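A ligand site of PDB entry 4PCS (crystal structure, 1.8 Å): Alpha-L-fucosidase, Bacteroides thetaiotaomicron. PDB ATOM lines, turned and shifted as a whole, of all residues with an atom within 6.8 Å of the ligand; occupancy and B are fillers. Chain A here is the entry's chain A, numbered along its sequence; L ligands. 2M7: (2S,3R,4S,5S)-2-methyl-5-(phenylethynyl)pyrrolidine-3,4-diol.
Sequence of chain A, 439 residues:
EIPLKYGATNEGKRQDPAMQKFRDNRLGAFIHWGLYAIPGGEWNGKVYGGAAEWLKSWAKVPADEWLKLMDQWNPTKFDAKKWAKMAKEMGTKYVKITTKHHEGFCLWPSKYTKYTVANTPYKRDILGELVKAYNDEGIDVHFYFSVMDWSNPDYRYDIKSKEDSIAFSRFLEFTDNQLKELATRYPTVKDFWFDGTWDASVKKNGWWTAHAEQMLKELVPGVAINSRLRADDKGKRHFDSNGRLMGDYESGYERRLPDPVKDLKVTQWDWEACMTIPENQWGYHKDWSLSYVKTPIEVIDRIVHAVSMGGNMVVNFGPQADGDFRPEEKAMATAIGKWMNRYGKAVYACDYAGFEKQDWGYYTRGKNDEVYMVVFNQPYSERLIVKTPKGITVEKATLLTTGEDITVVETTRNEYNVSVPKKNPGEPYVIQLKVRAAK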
ATOM      1  N   PHE A  30     -10.345 -16.297  25.647  1.00  0.00           N
ATOM      2  CA  PHE A  30      -9.852 -17.316  24.733  1.00  0.00           C
ATOM      3  C   PHE A  30      -8.360 -17.072  24.744  1.00  0.00           C
ATOM      4  O   PHE A  30      -7.943 -15.916  24.762  1.00  0.00           O
ATOM      5  CB  PHE A  30     -10.328 -17.100  23.291  1.00  0.00           C
ATOM      6  CG  PHE A  30     -10.822 -18.349  22.601  1.00  0.00           C
ATOM      7  CD1 PHE A  30     -10.049 -19.490  22.527  1.00  0.00           C
ATOM      8  CD2 PHE A  30     -12.084 -18.386  22.066  1.00  0.00           C
ATOM      9  CE1 PHE A  30     -10.546 -20.654  21.924  1.00  0.00           C
ATOM     10  CE2 PHE A  30     -12.582 -19.517  21.424  1.00  0.00           C
ATOM     11  CZ  PHE A  30     -11.821 -20.678  21.379  1.00  0.00           C
ATOM     12  N   HIS A  32      -5.113 -18.199  22.303  1.00  0.00           N
ATOM     13  CA  HIS A  32      -4.538 -18.839  21.132  1.00  0.00           C
ATOM     14  C   HIS A  32      -3.027 -18.696  21.276  1.00  0.00           C
ATOM     15  O   HIS A  32      -2.466 -17.620  21.102  1.00  0.00           O
ATOM     16  CB  HIS A  32      -5.002 -18.200  19.790  1.00  0.00           C
ATOM     17  CG  HIS A  32      -6.294 -18.731  19.270  1.00  0.00           C
ATOM     18  ND1 HIS A  32      -7.500 -18.459  19.870  1.00  0.00           N
ATOM     19  CD2 HIS A  32      -6.576 -19.553  18.223  1.00  0.00           C
ATOM     20  CE1 HIS A  32      -8.477 -19.076  19.221  1.00  0.00           C
ATOM     21  NE2 HIS A  32      -7.937 -19.789  18.242  1.00  0.00           N
ATOM     22  N   ALA A  51      -4.791 -14.091   9.242  1.00  0.00           N
ATOM     23  CA  ALA A  51      -4.689 -14.535  10.622  1.00  0.00           C
ATOM     24  C   ALA A  51      -3.356 -15.255  10.892  1.00  0.00           C
ATOM     25  O   ALA A  51      -2.983 -16.212  10.177  1.00  0.00           O
ATOM     26  CB  ALA A  51      -5.879 -15.408  10.991  1.00  0.00           C
ATOM     27  N   GLU A  53      -2.200 -17.278  13.014  1.00  0.00           N
ATOM     28  CA  GLU A  53      -2.210 -18.693  13.319  1.00  0.00           C
ATOM     29  C   GLU A  53      -2.373 -19.578  12.072  1.00  0.00           C
ATOM     30  O   GLU A  53      -2.201 -20.796  12.138  1.00  0.00           O
ATOM     31  CB  GLU A  53      -3.209 -19.051  14.414  1.00  0.00           C
ATOM     32  CG  GLU A  53      -4.699 -19.089  14.054  1.00  0.00           C
ATOM     33  CD  GLU A  53      -5.348 -17.717  13.841  1.00  0.00           C
ATOM     34  OE1 GLU A  53      -4.743 -16.667  14.157  1.00  0.00           O
ATOM     35  OE2 GLU A  53      -6.470 -17.749  13.280  1.00  0.00           O
ATOM     36  N   TRP A  54      -2.683 -18.934  10.947  1.00  0.00           N
ATOM     37  CA  TRP A  54      -2.810 -19.633   9.664  1.00  0.00           C
ATOM     38  C   TRP A  54      -1.593 -19.329   8.775  1.00  0.00           C
ATOM     39  O   TRP A  54      -1.623 -19.645   7.597  1.00  0.00           O
ATOM     40  CB  TRP A  54      -4.071 -19.178   8.948  1.00  0.00           C
ATOM     41  CG  TRP A  54      -5.252 -19.884   9.349  1.00  0.00           C
ATOM     42  CD1 TRP A  54      -5.950 -19.721  10.510  1.00  0.00           C
ATOM     43  CD2 TRP A  54      -5.935 -20.913   8.619  1.00  0.00           C
ATOM     44  NE1 TRP A  54      -7.024 -20.583  10.534  1.00  0.00           N
ATOM     45  CE2 TRP A  54      -7.022 -21.328   9.396  1.00  0.00           C
ATOM     46  CE3 TRP A  54      -5.738 -21.499   7.357  1.00  0.00           C
ATOM     47  CZ2 TRP A  54      -7.893 -22.335   8.978  1.00  0.00           C
ATOM     48  CZ3 TRP A  54      -6.581 -22.509   6.962  1.00  0.00           C
ATOM     49  CH2 TRP A  54      -7.652 -22.913   7.752  1.00  0.00           C
ATOM     50  N   THR A  98      -6.189 -23.142  23.665  1.00  0.00           N
ATOM     51  CA  THR A  98      -5.843 -23.996  22.513  1.00  0.00           C
ATOM     52  C   THR A  98      -4.877 -25.108  22.974  1.00  0.00           C
ATOM     53  O   THR A  98      -3.663 -24.878  23.067  1.00  0.00           O
ATOM     54  CB  THR A  98      -5.144 -23.207  21.390  1.00  0.00           C
ATOM     55  OG1 THR A  98      -4.076 -22.441  21.932  1.00  0.00           O
ATOM     56  CG2 THR A  98      -6.101 -22.267  20.653  1.00  0.00           C
ATOM     57  N   HIS A 101      -3.793 -26.478  17.947  1.00  0.00           N
ATOM     58  CA  HIS A 101      -4.392 -25.756  16.831  1.00  0.00           C
ATOM     59  C   HIS A 101      -4.112 -26.556  15.547  1.00  0.00           C
ATOM     60  O   HIS A 101      -3.626 -27.689  15.651  1.00  0.00           O
ATOM     61  CB  HIS A 101      -3.911 -24.278  16.784  1.00  0.00           C
ATOM     62  CG  HIS A 101      -4.875 -23.350  16.079  1.00  0.00           C
ATOM     63  ND1 HIS A 101      -4.727 -22.991  14.749  1.00  0.00           N
ATOM     64  CD2 HIS A 101      -6.052 -22.792  16.495  1.00  0.00           C
ATOM     65  CE1 HIS A 101      -5.728 -22.209  14.390  1.00  0.00           C
ATOM     66  NE2 HIS A 101      -6.559 -22.084  15.428  1.00  0.00           N
ATOM     67  N   HIS A 102      -4.437 -26.018  14.371  1.00  0.00           N
ATOM     68  CA  HIS A 102      -4.338 -26.777  13.119  1.00  0.00           C
ATOM     69  C   HIS A 102      -2.897 -27.251  12.881  1.00  0.00           C
ATOM     70  O   HIS A 102      -2.697 -28.339  12.335  1.00  0.00           O
ATOM     71  CB  HIS A 102      -4.797 -25.972  11.872  1.00  0.00           C
ATOM     72  CG  HIS A 102      -6.125 -25.295  12.020  1.00  0.00           C
ATOM     73  ND1 HIS A 102      -7.177 -25.832  12.747  1.00  0.00           N
ATOM     74  CD2 HIS A 102      -6.576 -24.113  11.517  1.00  0.00           C
ATOM     75  CE1 HIS A 102      -8.197 -24.988  12.722  1.00  0.00           C
ATOM     76  NE2 HIS A 102      -7.859 -23.954  11.975  1.00  0.00           N
ATOM     77  N   TYR A 144      -9.923 -26.038  23.806  1.00  0.00           N
ATOM     78  CA  TYR A 144     -10.092 -25.925  22.383  1.00  0.00           C
ATOM     79  C   TYR A 144      -9.270 -27.051  21.831  1.00  0.00           C
ATOM     80  O   TYR A 144      -8.157 -27.245  22.270  1.00  0.00           O
ATOM     81  CB  TYR A 144      -9.490 -24.594  21.893  1.00  0.00           C
ATOM     82  CG  TYR A 144      -9.270 -24.476  20.402  1.00  0.00           C
ATOM     83  CD1 TYR A 144      -8.277 -25.223  19.744  1.00  0.00           C
ATOM     84  CD2 TYR A 144     -10.008 -23.552  19.638  1.00  0.00           C
ATOM     85  CE1 TYR A 144      -8.044 -25.101  18.381  1.00  0.00           C
ATOM     86  CE2 TYR A 144      -9.802 -23.428  18.252  1.00  0.00           C
ATOM     87  CZ  TYR A 144      -8.849 -24.205  17.626  1.00  0.00           C
ATOM     88  OH  TYR A 144      -8.671 -24.122  16.282  1.00  0.00           O
ATOM     89  N   MET A 148      -8.742 -31.088  12.580  1.00  0.00           N
ATOM     90  CA  MET A 148      -7.776 -30.918  11.497  1.00  0.00           C
ATOM     91  C   MET A 148      -6.374 -30.743  12.069  1.00  0.00           C
ATOM     92  O   MET A 148      -6.162 -29.971  13.020  1.00  0.00           O
ATOM     93  CB  MET A 148      -8.138 -29.694  10.639  1.00  0.00           C
ATOM     94  CG  MET A 148      -7.197 -29.405   9.471  1.00  0.00           C
ATOM     95  SD  MET A 148      -7.764 -28.190   8.237  1.00  0.00           S
ATOM     96  CE  MET A 148      -7.595 -26.681   9.178  1.00  0.00           C
ATOM     97  N   TRP A 193     -14.135 -27.714  23.084  1.00  0.00           N
ATOM     98  CA  TRP A 193     -14.607 -26.853  22.021  1.00  0.00           C
ATOM     99  C   TRP A 193     -13.852 -27.274  20.777  1.00  0.00           C
ATOM    100  O   TRP A 193     -12.716 -26.877  20.572  1.00  0.00           O
ATOM    101  CB  TRP A 193     -14.323 -25.375  22.369  1.00  0.00           C
ATOM    102  CG  TRP A 193     -15.115 -24.378  21.521  1.00  0.00           C
ATOM    103  CD1 TRP A 193     -16.385 -23.922  21.769  1.00  0.00           C
ATOM    104  CD2 TRP A 193     -14.702 -23.778  20.279  1.00  0.00           C
ATOM    105  NE1 TRP A 193     -16.761 -23.068  20.758  1.00  0.00           N
ATOM    106  CE2 TRP A 193     -15.724 -22.932  19.863  1.00  0.00           C
ATOM    107  CE3 TRP A 193     -13.548 -23.878  19.493  1.00  0.00           C
ATOM    108  CZ2 TRP A 193     -15.656 -22.197  18.687  1.00  0.00           C
ATOM    109  CZ3 TRP A 193     -13.435 -23.100  18.354  1.00  0.00           C
ATOM    110  CH2 TRP A 193     -14.512 -22.325  17.920  1.00  0.00           C
ATOM    111  N   ASP A 195     -12.870 -27.452  16.818  1.00  0.00           N
ATOM    112  CA  ASP A 195     -12.683 -26.603  15.675  1.00  0.00           C
ATOM    113  C   ASP A 195     -12.082 -27.477  14.565  1.00  0.00           C
ATOM    114  O   ASP A 195     -11.720 -28.626  14.800  1.00  0.00           O
ATOM    115  CB  ASP A 195     -11.715 -25.466  15.992  1.00  0.00           C
ATOM    116  CG  ASP A 195     -11.909 -24.256  15.092  1.00  0.00           C
ATOM    117  OD1 ASP A 195     -12.877 -24.264  14.294  1.00  0.00           O
ATOM    118  OD2 ASP A 195     -11.056 -23.326  15.120  1.00  0.00           O
ATOM    119  N   GLY A 196     -11.986 -26.928  13.348  1.00  0.00           N
ATOM    120  CA  GLY A 196     -11.362 -27.623  12.230  1.00  0.00           C
ATOM    121  C   GLY A 196     -12.083 -28.924  11.871  1.00  0.00           C
ATOM    122  O   GLY A 196     -11.415 -29.917  11.568  1.00  0.00           O
ATOM    123  N   TRP A 198     -14.623 -29.058   9.519  1.00  0.00           N
ATOM    124  CA  TRP A 198     -15.426 -28.687   8.364  1.00  0.00           C
ATOM    125  C   TRP A 198     -15.118 -29.490   7.103  1.00  0.00           C
ATOM    126  O   TRP A 198     -15.911 -29.483   6.190  1.00  0.00           O
ATOM    127  CB  TRP A 198     -15.252 -27.200   8.026  1.00  0.00           C
ATOM    128  CG  TRP A 198     -13.869 -26.728   8.089  1.00  0.00           C
ATOM    129  CD1 TRP A 198     -12.860 -26.973   7.184  1.00  0.00           C
ATOM    130  CD2 TRP A 198     -13.298 -25.877   9.116  1.00  0.00           C
ATOM    131  NE1 TRP A 198     -11.694 -26.343   7.601  1.00  0.00           N
ATOM    132  CE2 TRP A 198     -11.935 -25.656   8.761  1.00  0.00           C
ATOM    133  CE3 TRP A 198     -13.803 -25.288  10.280  1.00  0.00           C
ATOM    134  CZ2 TRP A 198     -11.072 -24.875   9.549  1.00  0.00           C
ATOM    135  CZ3 TRP A 198     -12.931 -24.485  11.062  1.00  0.00           C
ATOM    136  CH2 TRP A 198     -11.580 -24.295  10.685  1.00  0.00           C
ATOM    137  N   ARG A 228     -20.058 -27.480  17.114  1.00  0.00           N
ATOM    138  CA  ARG A 228     -19.154 -27.458  15.967  1.00  0.00           C
ATOM    139  C   ARG A 228     -18.442 -28.791  15.714  1.00  0.00           C
ATOM    140  O   ARG A 228     -17.961 -29.078  14.607  1.00  0.00           O
ATOM    141  CB  ARG A 228     -18.086 -26.357  16.159  1.00  0.00           C
ATOM    142  CG  ARG A 228     -17.248 -26.149  14.919  1.00  0.00           C
ATOM    143  CD  ARG A 228     -16.332 -24.922  14.933  1.00  0.00           C
ATOM    144  NE  ARG A 228     -17.004 -23.641  15.272  1.00  0.00           N
ATOM    145  CZ  ARG A 228     -16.477 -22.431  15.044  1.00  0.00           C
ATOM    146  NH1 ARG A 228     -15.269 -22.300  14.471  1.00  0.00           N
ATOM    147  NH2 ARG A 228     -17.134 -21.323  15.433  1.00  0.00           N
ATOM    148  N   GLU A 254     -18.872 -16.554  15.368  1.00  0.00           N
ATOM    149  CA  GLU A 254     -17.471 -16.276  15.472  1.00  0.00           C
ATOM    150  C   GLU A 254     -17.136 -14.968  14.762  1.00  0.00           C
ATOM    151  O   GLU A 254     -17.310 -14.845  13.556  1.00  0.00           O
ATOM    152  CB  GLU A 254     -16.724 -17.473  14.846  1.00  0.00           C
ATOM    153  CG  GLU A 254     -15.227 -17.322  14.680  1.00  0.00           C
ATOM    154  CD  GLU A 254     -14.541 -18.628  14.275  1.00  0.00           C
ATOM    155  OE1 GLU A 254     -15.063 -19.699  14.624  1.00  0.00           O
ATOM    156  OE2 GLU A 254     -13.515 -18.569  13.578  1.00  0.00           O
ATOM    157  N   ARG A 255     -16.710 -13.955  15.526  1.00  0.00           N
ATOM    158  CA  ARG A 255     -16.557 -12.599  15.016  1.00  0.00           C
ATOM    159  C   ARG A 255     -17.863 -11.993  14.457  1.00  0.00           C
ATOM    160  O   ARG A 255     -17.818 -11.079  13.663  1.00  0.00           O
ATOM    161  CB  ARG A 255     -15.387 -12.494  14.023  1.00  0.00           C
ATOM    162  CG  ARG A 255     -14.092 -13.058  14.586  1.00  0.00           C
ATOM    163  CD  ARG A 255     -12.919 -12.892  13.621  1.00  0.00           C
ATOM    164  NE  ARG A 255     -13.273 -13.479  12.333  1.00  0.00           N
ATOM    165  CZ  ARG A 255     -13.434 -12.800  11.188  1.00  0.00           C
ATOM    166  NH1 ARG A 255     -13.225 -11.494  11.125  1.00  0.00           N
ATOM    167  NH2 ARG A 255     -13.777 -13.448  10.090  1.00  0.00           N
ATOM    168  N   CYS A 274     -17.617 -16.148  20.121  1.00  0.00           N
ATOM    169  CA  CYS A 274     -16.256 -15.748  20.360  1.00  0.00           C
ATOM    170  C   CYS A 274     -15.869 -14.600  19.473  1.00  0.00           C
ATOM    171  O   CYS A 274     -16.437 -14.418  18.421  1.00  0.00           O
ATOM    172  CB  CYS A 274     -15.297 -16.904  20.141  1.00  0.00           C
ATOM    173  SG  CYS A 274     -15.421 -17.795  18.603  1.00  0.00           S
ATOM    174  N   ASN A 280      -9.386  -9.744  12.485  1.00  0.00           N
ATOM    175  CA  ASN A 280      -9.216 -11.169  12.304  1.00  0.00           C
ATOM    176  C   ASN A 280      -7.778 -11.646  12.620  1.00  0.00           C
ATOM    177  O   ASN A 280      -7.012 -11.960  11.710  1.00  0.00           O
ATOM    178  CB  ASN A 280      -9.559 -11.539  10.868  1.00  0.00           C
ATOM    179  CG  ASN A 280      -9.823 -13.023  10.665  1.00  0.00           C
ATOM    180  OD1 ASN A 280      -9.728 -13.870  11.588  1.00  0.00           O
ATOM    181  ND2 ASN A 280     -10.175 -13.360   9.456  1.00  0.00           N
ATOM    182  N   TRP A 282      -6.204 -14.225  15.762  1.00  0.00           N
ATOM    183  CA  TRP A 282      -6.397 -14.999  16.964  1.00  0.00           C
ATOM    184  C   TRP A 282      -5.015 -15.296  17.624  1.00  0.00           C
ATOM    185  O   TRP A 282      -4.792 -14.919  18.779  1.00  0.00           O
ATOM    186  CB  TRP A 282      -7.117 -16.288  16.658  1.00  0.00           C
ATOM    187  CG  TRP A 282      -8.448 -16.112  16.027  1.00  0.00           C
ATOM    188  CD1 TRP A 282      -8.717 -16.051  14.704  1.00  0.00           C
ATOM    189  CD2 TRP A 282      -9.712 -16.104  16.696  1.00  0.00           C
ATOM    190  NE1 TRP A 282     -10.068 -15.969  14.498  1.00  0.00           N
ATOM    191  CE2 TRP A 282     -10.703 -15.995  15.711  1.00  0.00           C
ATOM    192  CE3 TRP A 282     -10.102 -16.153  18.021  1.00  0.00           C
ATOM    193  CZ2 TRP A 282     -12.061 -15.956  16.017  1.00  0.00           C
ATOM    194  CZ3 TRP A 282     -11.480 -16.094  18.336  1.00  0.00           C
ATOM    195  CH2 TRP A 282     -12.427 -16.003  17.335  1.00  0.00           C
ATOM    196  N   GLY A 283      -4.104 -15.924  16.873  1.00  0.00           N
ATOM    197  CA  GLY A 283      -2.727 -16.007  17.282  1.00  0.00           C
ATOM    198  C   GLY A 283      -2.088 -14.650  17.314  1.00  0.00           C
ATOM    199  O   GLY A 283      -2.571 -13.733  16.668  1.00  0.00           O
HETATM  200  CAI 2M7 L   1     -11.106 -21.188   8.570  1.00  0.00           C
HETATM  201  CAJ 2M7 L   1     -11.590 -21.147   7.265  1.00  0.00           C
HETATM  202  CAK 2M7 L   1     -12.746 -20.407   7.023  1.00  0.00           C
HETATM  203  CAL 2M7 L   1     -13.415 -19.723   8.065  1.00  0.00           C
HETATM  204  CAM 2M7 L   1     -12.919 -19.770   9.368  1.00  0.00           C
HETATM  205  CAH 2M7 L   1     -11.761 -20.525   9.610  1.00  0.00           C
HETATM  206  CAG 2M7 L   1     -11.166 -20.601  10.956  1.00  0.00           C
HETATM  207  CAF 2M7 L   1     -10.798 -20.653  12.011  1.00  0.00           C
HETATM  208  CAD 2M7 L   1     -10.225 -20.751  13.377  1.00  0.00           C
HETATM  209  NAE 2M7 L   1     -11.388 -20.642  14.285  1.00  0.00           N
HETATM  210  CAA 2M7 L   1     -11.057 -19.559  15.229  1.00  0.00           C
HETATM  211  CAN 2M7 L   1     -11.665 -19.769  16.582  1.00  0.00           C
HETATM  212  CAB 2M7 L   1      -9.567 -19.591  15.266  1.00  0.00           C
HETATM  213  OAO 2M7 L   1      -9.155 -20.821  15.918  1.00  0.00           O
HETATM  214  CAC 2M7 L   1      -9.350 -19.609  13.773  1.00  0.00           C
HETATM  215  OAP 2M7 L   1      -7.938 -19.759  13.447  1.00  0.00           O
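The side-chain carboxylate (OE2) of Glu 53 is in hydrogen-bond range of an oxygen (OAP) of the ligand (2.5 Å).
OAO of the ligand lies within hydrogen-bond range of NE2 of His 32 (2.8 Å).
NAE of the ligand lies within salt-bridge range of OD2 of Asp 195, at 2.8 Å.
An oxygen (OAO) of the ligand is in hydrogen-bond range of a ring nitrogen (NE2) of His 101 (2.9 Å).
OE2 of Glu 254 is in salt-bridge range of NAE of the ligand (3.1 Å).
OAP of the ligand lies within hydrogen-bond range of NE1 of Trp 54 (3.2 Å).
An oxygen (OAO) of the ligand is in hydrogen-bond range of the side-chain hydroxyl (OH) of Tyr 144.
N of Trp 282 sits at hydrogen-bond distance from OE1 of Glu 53 (3.3 Å).
The side-chain carboxylate (OE1) of Glu 53 is in hydrogen-bond range of the backbone NH (N) of Gly 283, 2.9 Å away.
The side-chain carboxylate of Asp 195 sits at hydrogen-bond distance from the side-chain hydroxyl of Tyr 144 (2.8 Å).
NH1 of Arg 228 lies within salt-bridge range of OD1 of Asp 195 (3.1 Å).
The side-chain hydroxyl of Tyr 144 lies close to a ring nitrogen (NE2) of His 101 (3.1 Å).
NH1 of Arg 228 is in salt-bridge range of OE1 of Glu 254 (2.6 Å).
CH2 of Trp 198 touches CAG of the ligand, at 3.7 Å.
Trp 282 touches the ligand (CE2 to CAA, 3.6 Å).
Nine residues have an atom within 4 Å of the ligand: His 32, Glu 53, Trp 54, His 101, Tyr 144, Asp 195, Trp 198, Glu 254 and Trp 282.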
